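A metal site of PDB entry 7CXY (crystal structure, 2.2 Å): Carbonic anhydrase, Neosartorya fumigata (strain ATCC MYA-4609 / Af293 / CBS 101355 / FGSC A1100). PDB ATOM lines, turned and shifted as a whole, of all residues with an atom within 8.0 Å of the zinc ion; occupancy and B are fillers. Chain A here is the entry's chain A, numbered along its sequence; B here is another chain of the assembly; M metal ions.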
ATOM      1  N   GLY A  56      20.203 -11.873  -1.758  1.00  0.00           N
ATOM      2  CA  GLY A  56      20.453 -11.152  -0.507  1.00  0.00           C
ATOM      3  C   GLY A  56      21.804 -10.502  -0.485  1.00  0.00           C
ATOM      4  O   GLY A  56      22.514 -10.603  -1.452  1.00  0.00           O
ATOM      5  N   CYS A  57      22.054  -9.759   0.563  1.00  0.00           N
ATOM      6  CA  CYS A  57      23.344  -9.066   0.716  1.00  0.00           C
ATOM      7  C   CYS A  57      24.395 -10.004   1.321  1.00  0.00           C
ATOM      8  O   CYS A  57      24.092 -10.753   2.182  1.00  0.00           O
ATOM      9  CB  CYS A  57      23.168  -7.855   1.603  1.00  0.00           C
ATOM     10  SG  CYS A  57      24.668  -6.872   1.748  1.00  0.00           S
ATOM     11  N   SER A  58      25.629  -9.830   0.871  1.00  0.00           N
ATOM     12  CA  SER A  58      26.835 -10.541   1.355  1.00  0.00           C
ATOM     13  C   SER A  58      27.088 -10.252   2.838  1.00  0.00           C
ATOM     14  O   SER A  58      27.520 -11.142   3.516  1.00  0.00           O
ATOM     15  CB  SER A  58      28.008 -10.158   0.504  1.00  0.00           C
ATOM     16  OG  SER A  58      27.954 -10.809  -0.738  1.00  0.00           O
ATOM     17  N   ASP A  59      26.798  -9.025   3.296  1.00  0.00           N
ATOM     18  CA  ASP A  59      27.104  -8.551   4.681  1.00  0.00           C
ATOM     19  C   ASP A  59      25.876  -8.681   5.582  1.00  0.00           C
ATOM     20  O   ASP A  59      25.970  -8.179   6.723  1.00  0.00           O
ATOM     21  CB  ASP A  59      27.702  -7.135   4.784  1.00  0.00           C
ATOM     22  CG  ASP A  59      26.837  -5.946   4.384  1.00  0.00           C
ATOM     23  OD1 ASP A  59      25.538  -5.809   4.862  1.00  0.00           O
ATOM     24  OD2 ASP A  59      27.269  -5.071   3.681  1.00  0.00           O
ATOM     25  N   SER A  60      24.807  -9.320   5.125  1.00  0.00           N
ATOM     26  CA  SER A  60      23.681  -9.745   5.988  1.00  0.00           C
ATOM     27  C   SER A  60      24.217 -10.912   6.825  1.00  0.00           C
ATOM     28  O   SER A  60      25.180 -11.565   6.347  1.00  0.00           O
ATOM     29  CB  SER A  60      22.403 -10.060   5.230  1.00  0.00           C
ATOM     30  OG  SER A  60      22.450 -11.305   4.550  1.00  0.00           O
ATOM     31  N   ARG A  61      23.616 -11.109   8.019  1.00  0.00           N
ATOM     32  CA  ARG A  61      24.264 -11.748   9.201  1.00  0.00           C
ATOM     33  C   ARG A  61      23.583 -13.073   9.551  1.00  0.00           C
ATOM     34  O   ARG A  61      24.004 -13.706  10.535  1.00  0.00           O
ATOM     35  CB  ARG A  61      24.186 -10.838  10.430  1.00  0.00           C
ATOM     36  CG  ARG A  61      25.062  -9.597  10.347  1.00  0.00           C
ATOM     37  CD  ARG A  61      24.728  -8.555  11.396  1.00  0.00           C
ATOM     38  NE  ARG A  61      24.653  -7.193  10.845  1.00  0.00           N
ATOM     39  CZ  ARG A  61      25.667  -6.349  10.738  1.00  0.00           C
ATOM     40  NH1 ARG A  61      25.476  -5.146  10.219  1.00  0.00           N
ATOM     41  NH2 ARG A  61      26.881  -6.696  11.156  1.00  0.00           N
ATOM     42  N   ASN A  80      25.353 -10.739  -2.753  1.00  0.00           N
ATOM     43  CA  ASN A  80      26.301  -9.780  -3.361  1.00  0.00           C
ATOM     44  C   ASN A  80      26.285  -8.514  -2.513  1.00  0.00           C
ATOM     45  O   ASN A  80      25.459  -8.430  -1.642  1.00  0.00           O
ATOM     46  CB  ASN A  80      25.997  -9.633  -4.856  1.00  0.00           C
ATOM     47  CG  ASN A  80      24.700  -8.920  -5.161  1.00  0.00           C
ATOM     48  OD1 ASN A  80      24.351  -7.961  -4.478  1.00  0.00           O
ATOM     49  ND2 ASN A  80      24.017  -9.325  -6.222  1.00  0.00           N
ATOM     50  N   ILE A  81      27.164  -7.550  -2.764  1.00  0.00           N
ATOM     51  CA  ILE A  81      27.189  -6.292  -1.958  1.00  0.00           C
ATOM     52  C   ILE A  81      25.902  -5.528  -2.248  1.00  0.00           C
ATOM     53  O   ILE A  81      25.718  -5.067  -3.419  1.00  0.00           O
ATOM     54  CB  ILE A  81      28.398  -5.386  -2.255  1.00  0.00           C
ATOM     55  CG1 ILE A  81      29.750  -6.093  -2.239  1.00  0.00           C
ATOM     56  CG2 ILE A  81      28.371  -4.169  -1.336  1.00  0.00           C
ATOM     57  CD1 ILE A  81      29.855  -7.033  -1.134  1.00  0.00           C
ATOM     58  N   ALA A  82      25.045  -5.391  -1.234  1.00  0.00           N
ATOM     59  CA  ALA A  82      23.853  -4.502  -1.258  1.00  0.00           C
ATOM     60  C   ALA A  82      22.733  -5.120  -2.082  1.00  0.00           C
ATOM     61  O   ALA A  82      21.849  -4.367  -2.498  1.00  0.00           O
ATOM     62  CB  ALA A  82      24.217  -3.129  -1.759  1.00  0.00           C
ATOM     63  N   ASN A  83      22.722  -6.445  -2.221  1.00  0.00           N
ATOM     64  CA  ASN A  83      21.600  -7.233  -2.827  1.00  0.00           C
ATOM     65  C   ASN A  83      21.132  -6.540  -4.113  1.00  0.00           C
ATOM     66  O   ASN A  83      19.935  -6.287  -4.267  1.00  0.00           O
ATOM     67  CB  ASN A  83      20.462  -7.530  -1.847  1.00  0.00           C
ATOM     68  CG  ASN A  83      20.017  -6.312  -1.028  1.00  0.00           C
ATOM     69  OD1 ASN A  83      20.566  -6.018   0.050  1.00  0.00           O
ATOM     70  ND2 ASN A  83      19.031  -5.587  -1.539  1.00  0.00           N
ATOM     71  N   CYS A 111      15.943  -9.813  -0.690  1.00  0.00           N
ATOM     72  CA  CYS A 111      15.900  -9.504   0.738  1.00  0.00           C
ATOM     73  C   CYS A 111      17.031  -8.541   1.077  1.00  0.00           C
ATOM     74  O   CYS A 111      18.175  -8.934   1.009  1.00  0.00           O
ATOM     75  CB  CYS A 111      15.934 -10.769   1.597  1.00  0.00           C
ATOM     76  SG  CYS A 111      15.626 -10.407   3.350  1.00  0.00           S
ATOM     77  N   GLY A 112      16.696  -7.338   1.496  1.00  0.00           N
ATOM     78  CA  GLY A 112      17.638  -6.362   2.057  1.00  0.00           C
ATOM     79  C   GLY A 112      17.655  -6.462   3.557  1.00  0.00           C
ATOM     80  O   GLY A 112      16.961  -7.322   4.111  1.00  0.00           O
ATOM     81  N   HIS A 113      18.433  -5.615   4.210  1.00  0.00           N
ATOM     82  CA  HIS A 113      18.539  -5.642   5.684  1.00  0.00           C
ATOM     83  C   HIS A 113      18.974  -4.253   6.101  1.00  0.00           C
ATOM     84  O   HIS A 113      19.669  -3.588   5.317  1.00  0.00           O
ATOM     85  CB  HIS A 113      19.433  -6.829   6.112  1.00  0.00           C
ATOM     86  CG  HIS A 113      20.855  -6.593   5.750  1.00  0.00           C
ATOM     87  ND1 HIS A 113      21.883  -6.661   6.695  1.00  0.00           N
ATOM     88  CD2 HIS A 113      21.414  -6.259   4.573  1.00  0.00           C
ATOM     89  CE1 HIS A 113      23.024  -6.368   6.115  1.00  0.00           C
ATOM     90  NE2 HIS A 113      22.733  -6.138   4.843  1.00  0.00           N
ATOM     91  N   TYR A 114      18.527  -3.804   7.272  1.00  0.00           N
ATOM     92  CA  TYR A 114      18.990  -2.540   7.885  1.00  0.00           C
ATOM     93  C   TYR A 114      20.416  -2.794   8.407  1.00  0.00           C
ATOM     94  O   TYR A 114      20.806  -3.963   8.533  1.00  0.00           O
ATOM     95  CB  TYR A 114      17.971  -2.053   8.937  1.00  0.00           C
ATOM     96  CG  TYR A 114      16.557  -1.848   8.436  1.00  0.00           C
ATOM     97  CD1 TYR A 114      16.294  -1.049   7.333  1.00  0.00           C
ATOM     98  CD2 TYR A 114      15.469  -2.428   9.085  1.00  0.00           C
ATOM     99  CE1 TYR A 114      14.994  -0.833   6.885  1.00  0.00           C
ATOM    100  CE2 TYR A 114      14.161  -2.229   8.647  1.00  0.00           C
ATOM    101  CZ  TYR A 114      13.921  -1.423   7.535  1.00  0.00           C
ATOM    102  OH  TYR A 114      12.659  -1.267   7.039  1.00  0.00           O
ATOM    103  N   HIS A 115      21.197  -1.745   8.639  1.00  0.00           N
ATOM    104  CA  HIS A 115      22.639  -1.838   9.017  1.00  0.00           C
ATOM    105  C   HIS A 115      23.396  -2.552   7.893  1.00  0.00           C
ATOM    106  O   HIS A 115      24.176  -3.490   8.173  1.00  0.00           O
ATOM    107  CB  HIS A 115      22.812  -2.502  10.388  1.00  0.00           C
ATOM    108  CG  HIS A 115      22.091  -1.768  11.458  1.00  0.00           C
ATOM    109  ND1 HIS A 115      20.871  -2.195  11.987  1.00  0.00           N
ATOM    110  CD2 HIS A 115      22.386  -0.595  12.064  1.00  0.00           C
ATOM    111  CE1 HIS A 115      20.477  -1.314  12.881  1.00  0.00           C
ATOM    112  NE2 HIS A 115      21.374  -0.325  12.955  1.00  0.00           N
ATOM    113  N   CYS A 116      23.130  -2.157   6.655  1.00  0.00           N
ATOM    114  CA  CYS A 116      23.732  -2.733   5.435  1.00  0.00           C
ATOM    115  C   CYS A 116      24.996  -1.958   5.163  1.00  0.00           C
ATOM    116  O   CYS A 116      24.868  -0.770   4.781  1.00  0.00           O
ATOM    117  CB  CYS A 116      22.788  -2.637   4.228  1.00  0.00           C
ATOM    118  SG  CYS A 116      23.566  -3.335   2.795  1.00  0.00           S
ATOM    119  N   GLY A 117      26.165  -2.567   5.361  1.00  0.00           N
ATOM    120  CA  GLY A 117      27.450  -1.912   5.106  1.00  0.00           C
ATOM    121  C   GLY A 117      27.572  -1.513   3.640  1.00  0.00           C
ATOM    122  O   GLY A 117      28.103  -0.451   3.366  1.00  0.00           O
ATOM    123  N   GLY A 118      27.056  -2.331   2.729  1.00  0.00           N
ATOM    124  CA  GLY A 118      27.045  -2.031   1.293  1.00  0.00           C
ATOM    125  C   GLY A 118      26.373  -0.709   0.985  1.00  0.00           C
ATOM    126  O   GLY A 118      26.988   0.151   0.325  1.00  0.00           O
ATOM    127  N   VAL A 119      25.140  -0.527   1.449  1.00  0.00           N
ATOM    128  CA  VAL A 119      24.349   0.705   1.170  1.00  0.00           C
ATOM    129  C   VAL A 119      25.015   1.899   1.868  1.00  0.00           C
ATOM    130  O   VAL A 119      25.062   2.970   1.243  1.00  0.00           O
ATOM    131  CB  VAL A 119      22.883   0.550   1.585  1.00  0.00           C
ATOM    132  CG1 VAL A 119      22.163   1.876   1.499  1.00  0.00           C
ATOM    133  CG2 VAL A 119      22.195  -0.532   0.743  1.00  0.00           C
ATOM    134  N   LYS A 120      25.514   1.721   3.094  1.00  0.00           N
ATOM    135  CA  LYS A 120      26.249   2.777   3.846  1.00  0.00           C
ATOM    136  C   LYS A 120      27.440   3.221   3.001  1.00  0.00           C
ATOM    137  O   LYS A 120      27.554   4.400   2.731  1.00  0.00           O
ATOM    138  CB  LYS A 120      26.729   2.267   5.219  1.00  0.00           C
ATOM    139  CG  LYS A 120      26.727   3.281   6.360  1.00  0.00           C
ATOM    140  CD  LYS A 120      28.038   3.442   7.183  1.00  0.00           C
ATOM    141  CE  LYS A 120      28.813   2.175   7.495  1.00  0.00           C
ATOM    142  NZ  LYS A 120      28.059   1.232   8.362  1.00  0.00           N
ATOM    143  N   VAL A 163      17.542   1.691   1.858  1.00  0.00           N
ATOM    144  CA  VAL A 163      17.585   0.202   1.863  1.00  0.00           C
ATOM    145  C   VAL A 163      16.301  -0.356   1.247  1.00  0.00           C
ATOM    146  O   VAL A 163      16.385  -1.330   0.492  1.00  0.00           O
ATOM    147  CB  VAL A 163      17.836  -0.348   3.288  1.00  0.00           C
ATOM    148  CG1 VAL A 163      17.590  -1.830   3.360  1.00  0.00           C
ATOM    149  CG2 VAL A 163      19.235   0.000   3.760  1.00  0.00           C
ATOM    150  N   ASN A 166      16.112   0.404  -2.559  1.00  0.00           N
ATOM    151  CA  ASN A 166      17.116  -0.488  -3.204  1.00  0.00           C
ATOM    152  C   ASN A 166      16.499  -1.863  -3.448  1.00  0.00           C
ATOM    153  O   ASN A 166      16.617  -2.382  -4.547  1.00  0.00           O
ATOM    154  CB  ASN A 166      18.400  -0.539  -2.379  1.00  0.00           C
ATOM    155  CG  ASN A 166      19.525  -1.184  -3.154  1.00  0.00           C
ATOM    156  OD1 ASN A 166      19.858  -0.724  -4.253  1.00  0.00           O
ATOM    157  ND2 ASN A 166      20.065  -2.250  -2.602  1.00  0.00           N
ATOM    158  N   PHE B  76      31.403 -13.417   5.727  1.00  0.00           N
ATOM    159  CA  PHE B  76      30.963 -12.617   4.562  1.00  0.00           C
ATOM    160  C   PHE B  76      30.805 -13.587   3.382  1.00  0.00           C
ATOM    161  O   PHE B  76      31.778 -14.331   3.116  1.00  0.00           O
ATOM    162  CB  PHE B  76      32.005 -11.545   4.294  1.00  0.00           C
ATOM    163  CG  PHE B  76      31.639 -10.481   3.304  1.00  0.00           C
ATOM    164  CD1 PHE B  76      30.664  -9.541   3.584  1.00  0.00           C
ATOM    165  CD2 PHE B  76      32.378 -10.338   2.144  1.00  0.00           C
ATOM    166  CE1 PHE B  76      30.366  -8.541   2.674  1.00  0.00           C
ATOM    167  CE2 PHE B  76      32.095  -9.316   1.245  1.00  0.00           C
ATOM    168  CZ  PHE B  76      31.089  -8.427   1.519  1.00  0.00           C
ATOM    169  N   TYR B  98      35.885  -5.500  -1.313  1.00  0.00           N
ATOM    170  CA  TYR B  98      35.239  -5.058  -0.053  1.00  0.00           C
ATOM    171  C   TYR B  98      35.767  -5.914   1.112  1.00  0.00           C
ATOM    172  O   TYR B  98      36.048  -5.361   2.186  1.00  0.00           O
ATOM    173  CB  TYR B  98      33.728  -5.187  -0.183  1.00  0.00           C
ATOM    174  CG  TYR B  98      32.943  -4.592   0.951  1.00  0.00           C
ATOM    175  CD1 TYR B  98      32.621  -3.246   0.956  1.00  0.00           C
ATOM    176  CD2 TYR B  98      32.447  -5.377   1.970  1.00  0.00           C
ATOM    177  CE1 TYR B  98      31.862  -2.679   1.979  1.00  0.00           C
ATOM    178  CE2 TYR B  98      31.679  -4.840   2.990  1.00  0.00           C
ATOM    179  CZ  TYR B  98      31.386  -3.486   2.994  1.00  0.00           C
ATOM    180  OH  TYR B  98      30.618  -2.941   3.999  1.00  0.00           O
HETATM  181 ZN    ZN M   1      24.160  -5.496   3.366  1.00  0.00          ZN
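Four residues have an atom within 4 Å of the zinc ion: Cys 57, Asp 59, His 113 and Cys 116.
The zinc ion is bound by the side-chain carboxylate (OD1) of Asp 59, a ring nitrogen (NE2) of His 113, the side-chain sulfur (SG) of Cys 57 and the side-chain sulfur (SG) of Cys 116.
The zinc ion has four donor atoms within binding distance.
The backbone NH of Gly 117 lies within hydrogen-bond range of the side-chain carboxylate of Asp 59 (3.2 Å).
The backbone NH of Gly 118 sits at hydrogen-bond distance from the side-chain carboxylate of Asp 59 (2.9 Å).
O of Cys 57 lies within hydrogen-bond range of OG of Ser 60 (2.9 Å).
The side-chain sulfur (SG) of Cys 57 lies close to the backbone NH (N) of Ala 82, 3.4 Å away.
SG of Cys 116 lies close to N of Gly 118 (3.6 Å).
SG of Cys 116 sits close to N of Val 119, 3.5 Å away.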
